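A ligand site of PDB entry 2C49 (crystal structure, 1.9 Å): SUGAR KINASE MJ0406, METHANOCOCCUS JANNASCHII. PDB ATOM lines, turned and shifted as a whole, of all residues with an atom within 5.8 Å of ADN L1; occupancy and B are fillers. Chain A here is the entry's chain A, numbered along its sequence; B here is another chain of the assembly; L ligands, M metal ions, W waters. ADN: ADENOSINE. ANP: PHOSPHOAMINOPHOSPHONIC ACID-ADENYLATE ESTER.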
ATOM      1  N   HIS A  13     -15.550  -0.335 -21.622  1.00  0.00           N
ATOM      2  CA  HIS A  13     -14.875   0.730 -22.355  1.00  0.00           C
ATOM      3  C   HIS A  13     -13.911   1.571 -21.534  1.00  0.00           C
ATOM      4  O   HIS A  13     -14.214   1.967 -20.402  1.00  0.00           O
ATOM      5  CB  HIS A  13     -15.905   1.702 -22.915  1.00  0.00           C
ATOM      6  CG  HIS A  13     -16.880   1.076 -23.872  1.00  0.00           C
ATOM      7  ND1 HIS A  13     -16.486   0.514 -25.068  1.00  0.00           N
ATOM      8  CD2 HIS A  13     -18.226   0.969 -23.807  1.00  0.00           C
ATOM      9  CE1 HIS A  13     -17.564   0.077 -25.704  1.00  0.00           C
ATOM     10  NE2 HIS A  13     -18.628   0.315 -24.943  1.00  0.00           N
ATOM     11  N   ALA A  15     -12.341   5.265 -22.708  1.00  0.00           N
ATOM     12  CA  ALA A  15     -12.768   6.226 -23.731  1.00  0.00           C
ATOM     13  C   ALA A  15     -12.270   7.618 -23.422  1.00  0.00           C
ATOM     14  O   ALA A  15     -11.924   7.885 -22.287  1.00  0.00           O
ATOM     15  CB  ALA A  15     -14.318   6.242 -23.832  1.00  0.00           C
ATOM     16  N   LEU A  16     -12.225   8.481 -24.444  1.00  0.00           N
ATOM     17  CA  LEU A  16     -12.015   9.916 -24.283  1.00  0.00           C
ATOM     18  C   LEU A  16     -13.367  10.639 -24.461  1.00  0.00           C
ATOM     19  O   LEU A  16     -14.120  10.373 -25.393  1.00  0.00           O
ATOM     20  CB  LEU A  16     -10.963  10.484 -25.270  1.00  0.00           C
ATOM     21  CG  LEU A  16      -9.569   9.940 -25.006  1.00  0.00           C
ATOM     22  CD1 LEU A  16      -8.611  10.223 -26.129  1.00  0.00           C
ATOM     23  CD2 LEU A  16      -9.010  10.448 -23.641  1.00  0.00           C
ATOM     24  N   ASP A  17     -13.661  11.516 -23.514  1.00  0.00           N
ATOM     25  CA  ASP A  17     -14.954  12.144 -23.373  1.00  0.00           C
ATOM     26  C   ASP A  17     -14.851  13.636 -23.659  1.00  0.00           C
ATOM     27  O   ASP A  17     -13.925  14.302 -23.141  1.00  0.00           O
ATOM     28  CB  ASP A  17     -15.385  12.080 -21.908  1.00  0.00           C
ATOM     29  CG  ASP A  17     -15.861  10.727 -21.473  1.00  0.00           C
ATOM     30  OD1 ASP A  17     -15.974   9.758 -22.288  1.00  0.00           O
ATOM     31  OD2 ASP A  17     -16.220  10.556 -20.287  1.00  0.00           O
ATOM     32  N   TYR A  41     -10.403  11.913 -19.632  1.00  0.00           N
ATOM     33  CA  TYR A  41     -10.277  10.496 -19.425  1.00  0.00           C
ATOM     34  C   TYR A  41     -11.639   9.949 -18.962  1.00  0.00           C
ATOM     35  O   TYR A  41     -12.254  10.480 -18.047  1.00  0.00           O
ATOM     36  CB  TYR A  41      -9.155  10.205 -18.412  1.00  0.00           C
ATOM     37  CG  TYR A  41      -7.755  10.678 -18.829  1.00  0.00           C
ATOM     38  CD1 TYR A  41      -6.873  11.206 -17.901  1.00  0.00           C
ATOM     39  CD2 TYR A  41      -7.328  10.566 -20.158  1.00  0.00           C
ATOM     40  CE1 TYR A  41      -5.573  11.639 -18.278  1.00  0.00           C
ATOM     41  CE2 TYR A  41      -6.050  10.978 -20.555  1.00  0.00           C
ATOM     42  CZ  TYR A  41      -5.170  11.505 -19.592  1.00  0.00           C
ATOM     43  OH  TYR A  41      -3.923  11.918 -19.977  1.00  0.00           O
ATOM     44  N   GLY A  42     -12.122   8.926 -19.648  1.00  0.00           N
ATOM     45  CA  GLY A  42     -13.478   8.431 -19.515  1.00  0.00           C
ATOM     46  C   GLY A  42     -13.613   6.956 -19.830  1.00  0.00           C
ATOM     47  O   GLY A  42     -12.605   6.236 -19.821  1.00  0.00           O
ATOM     48  N   GLY A  43     -14.842   6.527 -20.122  1.00  0.00           N
ATOM     49  CA  GLY A  43     -15.166   5.124 -20.323  1.00  0.00           C
ATOM     50  C   GLY A  43     -15.507   4.517 -18.967  1.00  0.00           C
ATOM     51  O   GLY A  43     -14.692   4.592 -18.035  1.00  0.00           O
ATOM     52  N   ALA A  44     -16.717   3.976 -18.846  1.00  0.00           N
ATOM     53  CA  ALA A  44     -17.203   3.381 -17.587  1.00  0.00           C
ATOM     54  C   ALA A  44     -16.272   2.416 -16.876  1.00  0.00           C
ATOM     55  O   ALA A  44     -16.138   2.458 -15.627  1.00  0.00           O
ATOM     56  CB  ALA A  44     -18.566   2.699 -17.786  1.00  0.00           C
ATOM     57  N   ASN A  47     -13.258   4.354 -15.668  1.00  0.00           N
ATOM     58  CA  ASN A  47     -13.647   5.308 -14.626  1.00  0.00           C
ATOM     59  C   ASN A  47     -13.724   4.565 -13.276  1.00  0.00           C
ATOM     60  O   ASN A  47     -13.270   5.051 -12.236  1.00  0.00           O
ATOM     61  CB  ASN A  47     -15.044   5.882 -14.920  1.00  0.00           C
ATOM     62  CG  ASN A  47     -15.070   6.909 -16.045  1.00  0.00           C
ATOM     63  OD1 ASN A  47     -14.029   7.503 -16.432  1.00  0.00           O
ATOM     64  ND2 ASN A  47     -16.290   7.140 -16.578  1.00  0.00           N
ATOM     65  N   ALA A  99     -16.730   9.624 -26.562  1.00  0.00           N
ATOM     66  CA  ALA A  99     -18.097   9.993 -26.171  1.00  0.00           C
ATOM     67  C   ALA A  99     -18.295  11.513 -26.275  1.00  0.00           C
ATOM     68  O   ALA A  99     -17.395  12.271 -25.921  1.00  0.00           O
ATOM     69  CB  ALA A  99     -18.366   9.497 -24.733  1.00  0.00           C
ATOM     70  N   ILE A 101     -20.966  14.044 -24.701  1.00  0.00           N
ATOM     71  CA  ILE A 101     -21.936  14.016 -23.598  1.00  0.00           C
ATOM     72  C   ILE A 101     -22.496  15.409 -23.385  1.00  0.00           C
ATOM     73  O   ILE A 101     -21.749  16.376 -23.181  1.00  0.00           O
ATOM     74  CB  ILE A 101     -21.219  13.486 -22.325  1.00  0.00           C
ATOM     75  CG1 ILE A 101     -20.681  12.064 -22.590  1.00  0.00           C
ATOM     76  CG2 ILE A 101     -22.166  13.530 -21.102  1.00  0.00           C
ATOM     77  CD1 ILE A 101     -19.648  11.576 -21.592  1.00  0.00           C
ATOM     78  N   THR A 111     -26.040  11.087 -24.922  1.00  0.00           N
ATOM     79  CA  THR A 111     -24.674  10.898 -25.369  1.00  0.00           C
ATOM     80  C   THR A 111     -24.650  10.288 -26.747  1.00  0.00           C
ATOM     81  O   THR A 111     -25.620   9.642 -27.171  1.00  0.00           O
ATOM     82  CB  THR A 111     -23.815  10.035 -24.387  1.00  0.00           C
ATOM     83  OG1 THR A 111     -24.182   8.651 -24.516  1.00  0.00           O
ATOM     84  CG2 THR A 111     -24.077  10.375 -22.900  1.00  0.00           C
ATOM     85  N   PHE A 112     -23.534  10.519 -27.416  1.00  0.00           N
ATOM     86  CA  PHE A 112     -23.201   9.918 -28.692  1.00  0.00           C
ATOM     87  C   PHE A 112     -21.883   9.208 -28.427  1.00  0.00           C
ATOM     88  O   PHE A 112     -20.976   9.821 -27.886  1.00  0.00           O
ATOM     89  CB  PHE A 112     -23.029  11.018 -29.739  1.00  0.00           C
ATOM     90  CG  PHE A 112     -24.257  11.905 -29.907  1.00  0.00           C
ATOM     91  CD1 PHE A 112     -24.480  13.010 -29.071  1.00  0.00           C
ATOM     92  CD2 PHE A 112     -25.163  11.663 -30.920  1.00  0.00           C
ATOM     93  CE1 PHE A 112     -25.592  13.845 -29.269  1.00  0.00           C
ATOM     94  CE2 PHE A 112     -26.256  12.487 -31.110  1.00  0.00           C
ATOM     95  CZ  PHE A 112     -26.482  13.573 -30.287  1.00  0.00           C
ATOM     96  N   PHE A 113     -21.783   7.933 -28.795  1.00  0.00           N
ATOM     97  CA  PHE A 113     -20.626   7.124 -28.450  1.00  0.00           C
ATOM     98  C   PHE A 113     -20.117   6.421 -29.703  1.00  0.00           C
ATOM     99  O   PHE A 113     -20.869   5.708 -30.375  1.00  0.00           O
ATOM    100  CB  PHE A 113     -20.978   6.135 -27.337  1.00  0.00           C
ATOM    101  CG  PHE A 113     -19.801   5.419 -26.767  1.00  0.00           C
ATOM    102  CD1 PHE A 113     -18.988   6.037 -25.812  1.00  0.00           C
ATOM    103  CD2 PHE A 113     -19.508   4.128 -27.179  1.00  0.00           C
ATOM    104  CE1 PHE A 113     -17.896   5.350 -25.258  1.00  0.00           C
ATOM    105  CE2 PHE A 113     -18.414   3.447 -26.652  1.00  0.00           C
ATOM    106  CZ  PHE A 113     -17.619   4.031 -25.662  1.00  0.00           C
ATOM    107  N   TRP A 115     -17.821   3.682 -31.275  1.00  0.00           N
ATOM    108  CA  TRP A 115     -17.467   2.344 -30.805  1.00  0.00           C
ATOM    109  C   TRP A 115     -15.989   2.026 -31.066  1.00  0.00           C
ATOM    110  O   TRP A 115     -15.362   1.388 -30.232  1.00  0.00           O
ATOM    111  CB  TRP A 115     -18.329   1.276 -31.521  1.00  0.00           C
ATOM    112  CG  TRP A 115     -18.528  -0.076 -30.799  1.00  0.00           C
ATOM    113  CD1 TRP A 115     -18.105  -1.312 -31.237  1.00  0.00           C
ATOM    114  CD2 TRP A 115     -19.233  -0.319 -29.579  1.00  0.00           C
ATOM    115  NE1 TRP A 115     -18.495  -2.304 -30.347  1.00  0.00           N
ATOM    116  CE2 TRP A 115     -19.190  -1.728 -29.327  1.00  0.00           C
ATOM    117  CE3 TRP A 115     -19.918   0.499 -28.666  1.00  0.00           C
ATOM    118  CZ2 TRP A 115     -19.778  -2.316 -28.200  1.00  0.00           C
ATOM    119  CZ3 TRP A 115     -20.506  -0.089 -27.539  1.00  0.00           C
ATOM    120  CH2 TRP A 115     -20.429  -1.482 -27.310  1.00  0.00           C
ATOM    121  N   THR A 138     -20.582  -1.334 -18.941  1.00  0.00           N
ATOM    122  CA  THR A 138     -20.821  -1.134 -20.386  1.00  0.00           C
ATOM    123  C   THR A 138     -20.074  -2.180 -21.205  1.00  0.00           C
ATOM    124  O   THR A 138     -19.555  -3.180 -20.647  1.00  0.00           O
ATOM    125  CB  THR A 138     -20.447   0.327 -20.887  1.00  0.00           C
ATOM    126  OG1 THR A 138     -19.044   0.564 -20.752  1.00  0.00           O
ATOM    127  CG2 THR A 138     -21.090   1.423 -19.997  1.00  0.00           C
ATOM    128  N   GLY A 139     -20.064  -1.950 -22.512  1.00  0.00           N
ATOM    129  CA  GLY A 139     -19.371  -2.737 -23.504  1.00  0.00           C
ATOM    130  C   GLY A 139     -20.234  -3.708 -24.294  1.00  0.00           C
ATOM    131  O   GLY A 139     -21.492  -3.658 -24.296  1.00  0.00           O
ATOM    132  N   GLN A 163     -25.071   2.714 -20.532  1.00  0.00           N
ATOM    133  CA  GLN A 163     -25.477   3.389 -21.752  1.00  0.00           C
ATOM    134  C   GLN A 163     -25.567   2.425 -22.927  1.00  0.00           C
ATOM    135  O   GLN A 163     -26.295   2.671 -23.877  1.00  0.00           O
ATOM    136  CB  GLN A 163     -24.493   4.533 -22.048  1.00  0.00           C
ATOM    137  CG  GLN A 163     -24.435   5.600 -20.926  1.00  0.00           C
ATOM    138  CD  GLN A 163     -23.271   5.439 -19.962  1.00  0.00           C
ATOM    139  OE1 GLN A 163     -22.784   6.440 -19.404  1.00  0.00           O
ATOM    140  NE2 GLN A 163     -22.858   4.202 -19.712  1.00  0.00           N
ATOM    141  N   ASP A 164     -24.846   1.296 -22.850  1.00  0.00           N
ATOM    142  CA  ASP A 164     -24.920   0.277 -23.919  1.00  0.00           C
ATOM    143  C   ASP A 164     -26.100  -0.704 -23.839  1.00  0.00           C
ATOM    144  O   ASP A 164     -26.276  -1.568 -24.695  1.00  0.00           O
ATOM    145  CB  ASP A 164     -23.623  -0.503 -23.976  1.00  0.00           C
ATOM    146  CG  ASP A 164     -22.508   0.310 -24.564  1.00  0.00           C
ATOM    147  OD1 ASP A 164     -22.780   1.225 -25.408  1.00  0.00           O
ATOM    148  OD2 ASP A 164     -21.342   0.095 -24.264  1.00  0.00           O
ATOM    149  N   THR A 243     -21.826  13.594 -14.768  1.00  0.00           N
ATOM    150  CA  THR A 243     -21.361  12.480 -15.605  1.00  0.00           C
ATOM    151  C   THR A 243     -20.652  11.330 -14.852  1.00  0.00           C
ATOM    152  O   THR A 243     -20.995  10.161 -15.011  1.00  0.00           O
ATOM    153  CB  THR A 243     -20.468  12.997 -16.756  1.00  0.00           C
ATOM    154  OG1 THR A 243     -21.155  14.038 -17.465  1.00  0.00           O
ATOM    155  CG2 THR A 243     -20.234  11.871 -17.827  1.00  0.00           C
ATOM    156  N   GLY A 244     -19.685  11.646 -14.006  1.00  0.00           N
ATOM    157  CA  GLY A 244     -18.961  10.574 -13.314  1.00  0.00           C
ATOM    158  C   GLY A 244     -19.701   9.941 -12.130  1.00  0.00           C
ATOM    159  O   GLY A 244     -19.196   8.985 -11.564  1.00  0.00           O
ATOM    160  N   ASP A 247     -20.516   5.727 -12.321  1.00  0.00           N
ATOM    161  CA  ASP A 247     -19.356   4.858 -12.164  1.00  0.00           C
ATOM    162  C   ASP A 247     -18.646   5.000 -10.819  1.00  0.00           C
ATOM    163  O   ASP A 247     -18.155   4.002 -10.285  1.00  0.00           O
ATOM    164  CB  ASP A 247     -18.380   5.038 -13.329  1.00  0.00           C
ATOM    165  CG  ASP A 247     -19.029   4.767 -14.652  1.00  0.00           C
ATOM    166  OD1 ASP A 247     -19.916   3.859 -14.710  1.00  0.00           O
ATOM    167  OD2 ASP A 247     -18.711   5.417 -15.666  1.00  0.00           O
ATOM    168  N   CYS A 283     -15.131  12.536 -15.549  1.00  0.00           N
ATOM    169  CA  CYS A 283     -15.488  11.422 -14.652  1.00  0.00           C
ATOM    170  C   CYS A 283     -14.446  11.002 -13.638  1.00  0.00           C
ATOM    171  O   CYS A 283     -14.775  10.316 -12.683  1.00  0.00           O
ATOM    172  CB  CYS A 283     -15.891  10.202 -15.453  1.00  0.00           C
ATOM    173  SG  CYS A 283     -17.427  10.412 -16.353  1.00  0.00           S
ATOM    174  N   SER B  31     -28.595   7.067 -24.990  1.00  0.00           N
ATOM    175  CA  SER B  31     -27.295   7.109 -25.640  1.00  0.00           C
ATOM    176  C   SER B  31     -27.442   6.382 -26.986  1.00  0.00           C
ATOM    177  O   SER B  31     -28.228   5.448 -27.114  1.00  0.00           O
ATOM    178  CB  SER B  31     -26.248   6.371 -24.803  1.00  0.00           C
ATOM    179  OG  SER B  31     -25.994   7.026 -23.557  1.00  0.00           O
ATOM    180  N   ILE B  32     -26.664   6.802 -27.965  1.00  0.00           N
ATOM    181  CA  ILE B  32     -26.520   5.982 -29.167  1.00  0.00           C
ATOM    182  C   ILE B  32     -25.061   5.626 -29.380  1.00  0.00           C
ATOM    183  O   ILE B  32     -24.161   6.389 -29.017  1.00  0.00           O
ATOM    184  CB  ILE B  32     -27.080   6.689 -30.438  1.00  0.00           C
ATOM    185  CG1 ILE B  32     -26.552   8.123 -30.524  1.00  0.00           C
ATOM    186  CG2 ILE B  32     -28.634   6.639 -30.474  1.00  0.00           C
ATOM    187  CD1 ILE B  32     -26.907   8.811 -31.897  1.00  0.00           C
ATOM    188  N   GLN B  33     -24.851   4.461 -29.975  1.00  0.00           N
ATOM    189  CA  GLN B  33     -23.523   3.984 -30.320  1.00  0.00           C
ATOM    190  C   GLN B  33     -23.394   3.830 -31.838  1.00  0.00           C
ATOM    191  O   GLN B  33     -24.299   3.324 -32.494  1.00  0.00           O
ATOM    192  CB  GLN B  33     -23.262   2.651 -29.625  1.00  0.00           C
ATOM    193  CG  GLN B  33     -23.342   2.736 -28.089  1.00  0.00           C
ATOM    194  CD  GLN B  33     -24.707   2.484 -27.541  1.00  0.00           C
ATOM    195  OE1 GLN B  33     -25.374   1.546 -27.979  1.00  0.00           O
ATOM    196  NE2 GLN B  33     -25.139   3.316 -26.574  1.00  0.00           N
HETATM  197  O5' ADN L   1     -20.468   6.327 -17.264  1.00  0.00           O
HETATM  198  C5' ADN L   1     -19.984   7.554 -17.798  1.00  0.00           C
HETATM  199  C4' ADN L   1     -19.117   7.179 -18.998  1.00  0.00           C
HETATM  200  O4' ADN L   1     -19.819   6.405 -19.977  1.00  0.00           O
HETATM  201  C3' ADN L   1     -18.234   8.211 -19.741  1.00  0.00           C
HETATM  202  O3' ADN L   1     -16.880   8.305 -19.300  1.00  0.00           O
HETATM  203  C2' ADN L   1     -18.337   7.863 -21.234  1.00  0.00           C
HETATM  204  O2' ADN L   1     -17.107   7.443 -21.837  1.00  0.00           O
HETATM  205  C1' ADN L   1     -19.270   6.650 -21.276  1.00  0.00           C
HETATM  206  N9  ADN L   1     -20.312   6.666 -22.282  1.00  0.00           N
HETATM  207  C8  ADN L   1     -21.110   7.699 -22.662  1.00  0.00           C
HETATM  208  N7  ADN L   1     -21.997   7.265 -23.614  1.00  0.00           N
HETATM  209  C5  ADN L   1     -21.792   5.956 -23.797  1.00  0.00           C
HETATM  210  C6  ADN L   1     -22.292   4.837 -24.599  1.00  0.00           C
HETATM  211  N6  ADN L   1     -23.292   5.069 -25.425  1.00  0.00           N
HETATM  212  N1  ADN L   1     -21.739   3.600 -24.496  1.00  0.00           N
HETATM  213  C2  ADN L   1     -20.729   3.310 -23.646  1.00  0.00           C
HETATM  214  N3  ADN L   1     -20.204   4.257 -22.842  1.00  0.00           N
HETATM  215  C4  ADN L   1     -20.713   5.594 -22.927  1.00  0.00           C
HETATM  216  PG  ANP L   2     -25.393   9.898 -16.253  1.00  0.00           P
HETATM  217  O1G ANP L   2     -23.887  10.189 -16.699  1.00  0.00           O
HETATM  218  O2G ANP L   2     -26.427  10.840 -16.993  1.00  0.00           O
HETATM  219  O3G ANP L   2     -25.712   8.384 -16.644  1.00  0.00           O
HETATM  220  PB  ANP L   2     -26.949   9.313 -13.840  1.00  0.00           P
HETATM  221  O1B ANP L   2     -28.296   9.778 -14.553  1.00  0.00           O
HETATM  222  O2B ANP L   2     -26.593   7.813 -14.299  1.00  0.00           O
HETATM  223  N3B ANP L   2     -25.606  10.186 -14.532  1.00  0.00           N
HETATM  224  PA  ANP L   2     -26.984   8.253 -11.247  1.00  0.00           P
HETATM  225  O1A ANP L   2     -28.342   7.449 -10.978  1.00  0.00           O
HETATM  226  O2A ANP L   2     -25.880   7.259 -11.826  1.00  0.00           O
HETATM  227  O3A ANP L   2     -27.104   9.536 -12.223  1.00  0.00           O
HETATM  228  O5' ANP L   2     -26.445   8.787  -9.827  1.00  0.00           O
HETATM  229  C5' ANP L   2     -25.595   7.863  -9.186  1.00  0.00           C
HETATM  230  C4' ANP L   2     -25.422   8.256  -7.735  1.00  0.00           C
HETATM  231  O4' ANP L   2     -24.496   9.340  -7.540  1.00  0.00           O
HETATM  232  C3' ANP L   2     -26.672   8.556  -6.913  1.00  0.00           C
HETATM  233  O3' ANP L   2     -27.360   7.466  -6.353  1.00  0.00           O
HETATM  234  C2' ANP L   2     -26.278   9.692  -6.000  1.00  0.00           C
HETATM  235  O2' ANP L   2     -25.892   9.095  -4.757  1.00  0.00           O
HETATM  236  C1' ANP L   2     -24.945  10.220  -6.520  1.00  0.00           C
HETATM  237  N9  ANP L   2     -25.337  11.530  -7.101  1.00  0.00           N
HETATM  238  C8  ANP L   2     -25.990  11.779  -8.269  1.00  0.00           C
HETATM  239  N7  ANP L   2     -26.239  13.108  -8.499  1.00  0.00           N
HETATM  240  C5  ANP L   2     -25.737  13.726  -7.427  1.00  0.00           C
HETATM  241  C6  ANP L   2     -25.607  15.107  -6.921  1.00  0.00           C
HETATM  242  N6  ANP L   2     -26.105  16.090  -7.706  1.00  0.00           N
HETATM  243  N1  ANP L   2     -24.986  15.338  -5.725  1.00  0.00           N
HETATM  244  C2  ANP L   2     -24.476  14.367  -4.937  1.00  0.00           C
HETATM  245  N3  ANP L   2     -24.524  13.057  -5.289  1.00  0.00           N
HETATM  246  C4  ANP L   2     -25.177  12.720  -6.547  1.00  0.00           C
HETATM  247 MG    MG M   1     -23.914   4.440 -15.682  1.00  0.00          MG
HETATM  248  O   HOH W   1     -18.260   3.284 -21.140  1.00  0.00           O
HETATM  249  O   HOH W   2     -22.645   6.196 -15.878  1.00  0.00           O
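Water W1 lies within hydrogen-bond range of a nitrogen (N3) of ADN L1, the backbone NH (N) of Ala 44 and the side-chain hydroxyl (OG1) of Thr 138.
His 13 touches ADN L1.
Ala 15 touches ADN L1 (CB to O2', 3.6 Å).
Gly 42 touches ADN L1 (CA to O3', 3.4 Å).
CB of Ala 99 touches O2' of ADN L1 (3.8 Å).
Ile 101 touches ADN L1 (CD1 to C2', 3.95 Å).
Phe 113 touches ADN L1.
O of Thr 243 touches C5' of ADN L1, 3.9 Å away.
CB of Ser 31 of chain B touches N6 of ADN L1 (3.3 Å).
O of Ile 32 of chain B touches N6 of ADN L1 (3.9 Å).
Hydrophobic or aromatic side chains within 4 Å of ADN L1: His 13, Ala 15, Ala 99, Ile 101 and Phe 113.
Within 4 Å of ADN L1: His 13, Ala 15, Asp 17, Gly 42, Gly 43, Asn 47, Ala 99, Ile 101, Thr 111, Phe 113, Gln 163, Asp 164, Thr 243, Asp 247, Cys 283, Ser 31 of chain B, Ile 32 of chain B and Gln 33 of chain B.
The backbone carbonyl oxygen (O) of Ile 32 of chain B lies within hydrogen-bond range of the backbone NH (N) of Phe 113 (2.8 Å).
The side-chain hydroxyl of Thr 111 sits at hydrogen-bond distance from the side-chain hydroxyl of Ser 31 of chain B (2.6 Å).
ND2 of Asn 47 sits close to O of Gly 43.
The backbone NH (N) of Gly 42 lies within hydrogen-bond range of the backbone carbonyl oxygen (O) of Ala 15, 2.8 Å away.
NE2 of Gln 33 of chain B sits at hydrogen-bond distance from O of Gln 163, at 3.0 Å.
The side-chain carboxylate of Asp 164 lies close to the side-chain amide nitrogen of Gln 33 of chain B (3.4 Å).
OD2 of Asp 164 sits at hydrogen-bond distance from NE2 of His 13 (2.8 Å).
ND2 of Asn 47 is in hydrogen-bond range of OD2 of Asp 247, 3.1 Å away.
OD1 of Asp 164 is in hydrogen-bond range of N1 of ADN L1 (2.7 Å).
An oxygen (O3') of ADN L1 is in hydrogen-bond range of the backbone NH (N) of Gly 43 (2.8 Å).
O3' of ADN L1 sits at hydrogen-bond distance from OD2 of Asp 17.
The side-chain carboxylate (OD2) of Asp 247 lies within hydrogen-bond range of an oxygen (O5') of ADN L1 (2.5 Å).
A nitrogen (N7) of ADN L1 sits at hydrogen-bond distance from the side-chain hydroxyl (OG1) of Thr 111 (2.7 Å).
The side-chain amide nitrogen (NE2) of Gln 33 of chain B lies close to a nitrogen (N6) of ADN L1, at 2.8 Å.
The side-chain amide nitrogen of Asn 47 is in hydrogen-bond range of an oxygen (O3') of ADN L1, 3.0 Å away.
SG of Cys 283 is in hydrogen-bond range of O3' of ADN L1, 3.7 Å away.
OE1 of Gln 163 sits close to O4' of ADN L1 (3.0 Å).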
